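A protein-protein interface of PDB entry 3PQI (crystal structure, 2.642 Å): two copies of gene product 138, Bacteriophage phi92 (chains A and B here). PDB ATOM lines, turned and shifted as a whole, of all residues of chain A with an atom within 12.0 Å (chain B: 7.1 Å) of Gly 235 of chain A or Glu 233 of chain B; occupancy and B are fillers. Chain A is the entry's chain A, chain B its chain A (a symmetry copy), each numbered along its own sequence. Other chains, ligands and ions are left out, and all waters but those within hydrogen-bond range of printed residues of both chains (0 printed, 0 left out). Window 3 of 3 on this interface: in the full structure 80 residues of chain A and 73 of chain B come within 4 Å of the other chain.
N of Glu 233 of chain B lies within hydrogen-bond range of O of Glu 233 of chain A. The backbone NH (N) of Gly 235 of chain A sits at hydrogen-bond distance from the backbone carbonyl oxygen (O) of Gly 231 of chain B. The backbone NH of Gly 236 of chain A lies within hydrogen-bond range of the backbone carbonyl oxygen of Val 232 of chain B (3.4 Å). The backbone carbonyl oxygen (O) of Ser 237 of chain A lies within hydrogen-bond range of the backbone NH (N) of Gly 231 of chain B. O of Val 232 of chain B lies within hydrogen-bond range of N of Ser 237 of chain A. N of Val 232 of chain B sits close to N of Gly 235 of chain A (3.5 Å).
Among the printed residues, merely in contact across the chains: Glu 233 of chain A with Val 232 of chain B (3.5 Å), Thr 234 of chain A with Gly 231 of chain B (3.8 Å), Gly 235 of chain A with Glu 233 of chain B (3.8 Å), Ser 237 of chain A with Arg 230 of chain B (3.7 Å), Ser 237 of chain A with Thr 234 of chain B (3.4 Å), Thr 238 of chain A with Arg 230 of chain B (3.1 Å) and Thr 238 of chain A with Gly 231 of chain B (3.7 Å).
Thr 234 of chain A touches Gly 231 of chain B, but with the chains exchanged Gly 231 of chain A does not touch Thr 234 of chain B (11.0 Å). Gly 235 of chain A touches Gly 231 of chain B, but with the chains exchanged Gly 231 of chain A does not touch Gly 235 of chain B (10.2 Å). Gly 235 of chain A touches Val 232 of chain B, but with the chains exchanged Val 232 of chain A does not touch Gly 235 of chain B (9.0 Å). Gly 236 of chain A touches Val 232 of chain B, but with the chains exchanged Val 232 of chain A does not touch Gly 236 of chain B (10.1 Å). Positions printed for both chains: 230, 231, 232, 233, 234, 235 and 236. Of the 13 pairs that touch across the chains among the printed residues, 1 has its exchanged pair printed and touching as well.
Of the printed residues of chain B, Glu 233 of chain A touches Val 232 (3.5 Å) and Glu 233 (3.2 Å). Of the printed residues of chain B, Ser 237 of chain A touches Arg 230, Gly 231, Val 232 and Thr 234. Of the printed residues of chain A, Arg 230 of chain B touches Ser 237 and Thr 238. Printed residues of chain A within 4 Å of Gly 231 of chain B: Thr 234, Gly 235, Ser 237 and Thr 238. Val 232 of chain B touches just these residues of chain A: Glu 233 (3.5 Å), Gly 235 (3.3 Å), Gly 236 (3.4 Å) and Ser 237 (2.9 Å). Glu 233 of chain B touches just these residues of chain A: Glu 233 and Gly 235. Of chain A, only Ser 237 comes within 4 Å of Thr 234 of chain B. No residue of chain A comes within 4 Å of Gly 235 of chain B.
Of the 12 printed residues of chain A, 6 touch a printed residue of chain B. Hydrophobic or aromatic side chains of chain B within 4 Å of the printed part of chain A: Val 232. Among the printed residues, 13 pairs touch across the chains. Among the printed residues, no Asp or Glu carboxylate lies within 4 Å of a Lys or Arg side-chain nitrogen of the other chain.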
ATOM      1  N   VAL A 229       5.131  21.069  11.924  1.00  0.00           N
ATOM      2  CA  VAL A 229       5.227  19.806  12.653  1.00  0.00           C
ATOM      3  C   VAL A 229       5.104  20.030  14.161  1.00  0.00           C
ATOM      4  O   VAL A 229       5.818  20.851  14.734  1.00  0.00           O
ATOM      5  CB  VAL A 229       6.556  19.086  12.354  1.00  0.00           C
ATOM      6  CG1 VAL A 229       6.563  17.704  12.987  1.00  0.00           C
ATOM      7  CG2 VAL A 229       6.781  18.988  10.852  1.00  0.00           C
ATOM      8  N   ARG A 230       4.206  19.286  14.802  1.00  0.00           N
ATOM      9  CA  ARG A 230       3.897  19.499  16.216  1.00  0.00           C
ATOM     10  C   ARG A 230       4.495  18.443  17.148  1.00  0.00           C
ATOM     11  O   ARG A 230       4.714  17.297  16.750  1.00  0.00           O
ATOM     12  CB  ARG A 230       2.382  19.558  16.412  1.00  0.00           C
ATOM     13  CG  ARG A 230       1.711  20.739  15.734  1.00  0.00           C
ATOM     14  CD  ARG A 230       0.321  20.370  15.243  1.00  0.00           C
ATOM     15  NE  ARG A 230      -0.453  19.653  16.254  1.00  0.00           N
ATOM     16  CZ  ARG A 230      -1.264  20.239  17.130  1.00  0.00           C
ATOM     17  NH1 ARG A 230      -1.409  21.556  17.126  1.00  0.00           N
ATOM     18  NH2 ARG A 230      -1.928  19.504  18.013  1.00  0.00           N
ATOM     19  N   GLY A 231       4.752  18.844  18.391  1.00  0.00           N
ATOM     20  CA  GLY A 231       5.205  17.934  19.429  1.00  0.00           C
ATOM     21  C   GLY A 231       6.581  17.325  19.229  1.00  0.00           C
ATOM     22  O   GLY A 231       6.706  16.112  19.061  1.00  0.00           O
ATOM     23  N   VAL A 232       7.617  18.159  19.253  1.00  0.00           N
ATOM     24  CA  VAL A 232       8.994  17.678  19.135  1.00  0.00           C
ATOM     25  C   VAL A 232       9.952  18.490  20.006  1.00  0.00           C
ATOM     26  O   VAL A 232       9.612  19.576  20.474  1.00  0.00           O
ATOM     27  CB  VAL A 232       9.495  17.727  17.673  1.00  0.00           C
ATOM     28  CG1 VAL A 232       8.622  16.861  16.777  1.00  0.00           C
ATOM     29  CG2 VAL A 232       9.536  19.163  17.169  1.00  0.00           C
ATOM     30  N   GLU A 233      11.150  17.954  20.226  1.00  0.00           N
ATOM     31  CA  GLU A 233      12.185  18.661  20.979  1.00  0.00           C
ATOM     32  C   GLU A 233      13.072  19.482  20.049  1.00  0.00           C
ATOM     33  O   GLU A 233      13.803  18.924  19.228  1.00  0.00           O
ATOM     34  CB  GLU A 233      13.039  17.677  21.787  1.00  0.00           C
ATOM     35  CG  GLU A 233      14.371  18.250  22.284  1.00  0.00           C
ATOM     36  CD  GLU A 233      14.198  19.352  23.316  1.00  0.00           C
ATOM     37  OE1 GLU A 233      13.089  19.472  23.879  1.00  0.00           O
ATOM     38  OE2 GLU A 233      15.169  20.099  23.564  1.00  0.00           O
ATOM     39  N   THR A 234      13.004  20.806  20.175  1.00  0.00           N
ATOM     40  CA  THR A 234      13.886  21.683  19.412  1.00  0.00           C
ATOM     41  C   THR A 234      15.326  21.221  19.589  1.00  0.00           C
ATOM     42  O   THR A 234      15.878  21.291  20.686  1.00  0.00           O
ATOM     43  CB  THR A 234      13.777  23.157  19.863  1.00  0.00           C
ATOM     44  OG1 THR A 234      14.094  23.261  21.257  1.00  0.00           O
ATOM     45  CG2 THR A 234      12.375  23.696  19.621  1.00  0.00           C
ATOM     46  N   GLY A 235      15.930  20.738  18.510  1.00  0.00           N
ATOM     47  CA  GLY A 235      17.284  20.219  18.569  1.00  0.00           C
ATOM     48  C   GLY A 235      18.231  20.913  17.612  1.00  0.00           C
ATOM     49  O   GLY A 235      18.075  22.096  17.316  1.00  0.00           O
ATOM     50  N   GLY A 236      19.221  20.168  17.132  1.00  0.00           N
ATOM     51  CA  GLY A 236      20.196  20.697  16.198  1.00  0.00           C
ATOM     52  C   GLY A 236      20.415  19.754  15.030  1.00  0.00           C
ATOM     53  O   GLY A 236      21.315  19.956  14.215  1.00  0.00           O
ATOM     54  N   SER A 237      19.584  18.717  14.959  1.00  0.00           N
ATOM     55  CA  SER A 237      19.659  17.729  13.889  1.00  0.00           C
ATOM     56  C   SER A 237      18.605  17.992  12.820  1.00  0.00           C
ATOM     57  O   SER A 237      17.723  18.831  12.997  1.00  0.00           O
ATOM     58  CB  SER A 237      19.489  16.315  14.447  1.00  0.00           C
ATOM     59  OG  SER A 237      20.441  16.036  15.452  1.00  0.00           O
ATOM     60  N   THR A 238      18.696  17.258  11.716  1.00  0.00           N
ATOM     61  CA  THR A 238      17.770  17.427  10.601  1.00  0.00           C
ATOM     62  C   THR A 238      17.443  16.094   9.927  1.00  0.00           C
ATOM     63  O   THR A 238      18.323  15.430   9.378  1.00  0.00           O
ATOM     64  CB  THR A 238      18.325  18.418   9.552  1.00  0.00           C
ATOM     65  OG1 THR A 238      18.212  19.758  10.051  1.00  0.00           O
ATOM     66  CG2 THR A 238      17.559  18.304   8.243  1.00  0.00           C
ATOM     67  N   VAL A 239      16.172  15.703   9.982  1.00  0.00           N
ATOM     68  CA  VAL A 239      15.717  14.480   9.329  1.00  0.00           C
ATOM     69  C   VAL A 239      14.763  14.801   8.183  1.00  0.00           C
ATOM     70  O   VAL A 239      14.184  15.886   8.132  1.00  0.00           O
ATOM     71  CB  VAL A 239      15.022  13.519  10.320  1.00  0.00           C
ATOM     72  CG1 VAL A 239      16.034  12.935  11.296  1.00  0.00           C
ATOM     73  CG2 VAL A 239      13.898  14.232  11.061  1.00  0.00           C
ATOM     74  N   THR A 240      14.608  13.855   7.264  1.00  0.00           N
ATOM     75  CA  THR A 240      13.712  14.034   6.130  1.00  0.00           C
ATOM     76  C   THR A 240      12.489  13.135   6.276  1.00  0.00           C
ATOM     77  O   THR A 240      12.612  11.947   6.578  1.00  0.00           O
ATOM     78  CB  THR A 240      14.421  13.732   4.797  1.00  0.00           C
ATOM     79  OG1 THR A 240      14.913  12.386   4.810  1.00  0.00           O
ATOM     80  CG2 THR A 240      15.587  14.690   4.582  1.00  0.00           C
ATOM     81  N   ARG B 230      14.348  20.774   9.889  1.00  0.00           N
ATOM     82  CA  ARG B 230      15.533  21.271  10.586  1.00  0.00           C
ATOM     83  C   ARG B 230      15.320  21.502  12.084  1.00  0.00           C
ATOM     84  O   ARG B 230      14.205  21.773  12.532  1.00  0.00           O
ATOM     85  CB  ARG B 230      16.014  22.567   9.931  1.00  0.00           C
ATOM     86  CG  ARG B 230      16.503  22.399   8.504  1.00  0.00           C
ATOM     87  CD  ARG B 230      16.188  23.631   7.670  1.00  0.00           C
ATOM     88  NE  ARG B 230      16.542  24.871   8.356  1.00  0.00           N
ATOM     89  CZ  ARG B 230      17.715  25.483   8.238  1.00  0.00           C
ATOM     90  NH1 ARG B 230      18.659  24.969   7.460  1.00  0.00           N
ATOM     91  NH2 ARG B 230      17.947  26.609   8.900  1.00  0.00           N
ATOM     92  N   GLY B 231      16.405  21.390  12.848  1.00  0.00           N
ATOM     93  CA  GLY B 231      16.397  21.697  14.268  1.00  0.00           C
ATOM     94  C   GLY B 231      15.558  20.784  15.144  1.00  0.00           C
ATOM     95  O   GLY B 231      14.573  21.223  15.738  1.00  0.00           O
ATOM     96  N   VAL B 232      15.947  19.514  15.234  1.00  0.00           N
ATOM     97  CA  VAL B 232      15.254  18.558  16.097  1.00  0.00           C
ATOM     98  C   VAL B 232      16.226  17.569  16.740  1.00  0.00           C
ATOM     99  O   VAL B 232      17.373  17.445  16.310  1.00  0.00           O
ATOM    100  CB  VAL B 232      14.179  17.760  15.323  1.00  0.00           C
ATOM    101  CG1 VAL B 232      13.134  18.698  14.735  1.00  0.00           C
ATOM    102  CG2 VAL B 232      14.822  16.912  14.234  1.00  0.00           C
ATOM    103  N   GLU B 233      15.764  16.870  17.773  1.00  0.00           N
ATOM    104  CA  GLU B 233      16.567  15.840  18.428  1.00  0.00           C
ATOM    105  C   GLU B 233      16.318  14.472  17.800  1.00  0.00           C
ATOM    106  O   GLU B 233      15.218  13.928  17.901  1.00  0.00           O
ATOM    107  CB  GLU B 233      16.268  15.788  19.931  1.00  0.00           C
ATOM    108  CG  GLU B 233      16.742  14.510  20.631  1.00  0.00           C
ATOM    109  CD  GLU B 233      18.254  14.373  20.663  1.00  0.00           C
ATOM    110  OE1 GLU B 233      18.949  15.385  20.430  1.00  0.00           O
ATOM    111  OE2 GLU B 233      18.749  13.254  20.921  1.00  0.00           O
ATOM    112  N   THR B 234      17.340  13.923  17.147  1.00  0.00           N
ATOM    113  CA  THR B 234      17.247  12.573  16.599  1.00  0.00           C
ATOM    114  C   THR B 234      16.758  11.624  17.686  1.00  0.00           C
ATOM    115  O   THR B 234      17.452  11.390  18.674  1.00  0.00           O
ATOM    116  CB  THR B 234      18.606  12.063  16.068  1.00  0.00           C
ATOM    117  OG1 THR B 234      19.576  12.080  17.123  1.00  0.00           O
ATOM    118  CG2 THR B 234      19.095  12.925  14.915  1.00  0.00           C
ATOM    119  N   GLY B 235      15.557  11.089  17.508  1.00  0.00           N
ATOM    120  CA  GLY B 235      14.964  10.213  18.500  1.00  0.00           C
ATOM    121  C   GLY B 235      14.596   8.851  17.951  1.00  0.00           C
ATOM    122  O   GLY B 235      15.247   8.340  17.041  1.00  0.00           O
ATOM    123  N   GLY B 236      13.547   8.260  18.514  1.00  0.00           N
ATOM    124  CA  GLY B 236      13.077   6.959  18.082  1.00  0.00           C
ATOM    125  C   GLY B 236      11.571   6.948  17.896  1.00  0.00           C
ATOM    126  O   GLY B 236      10.968   5.896  17.681  1.00  0.00           O
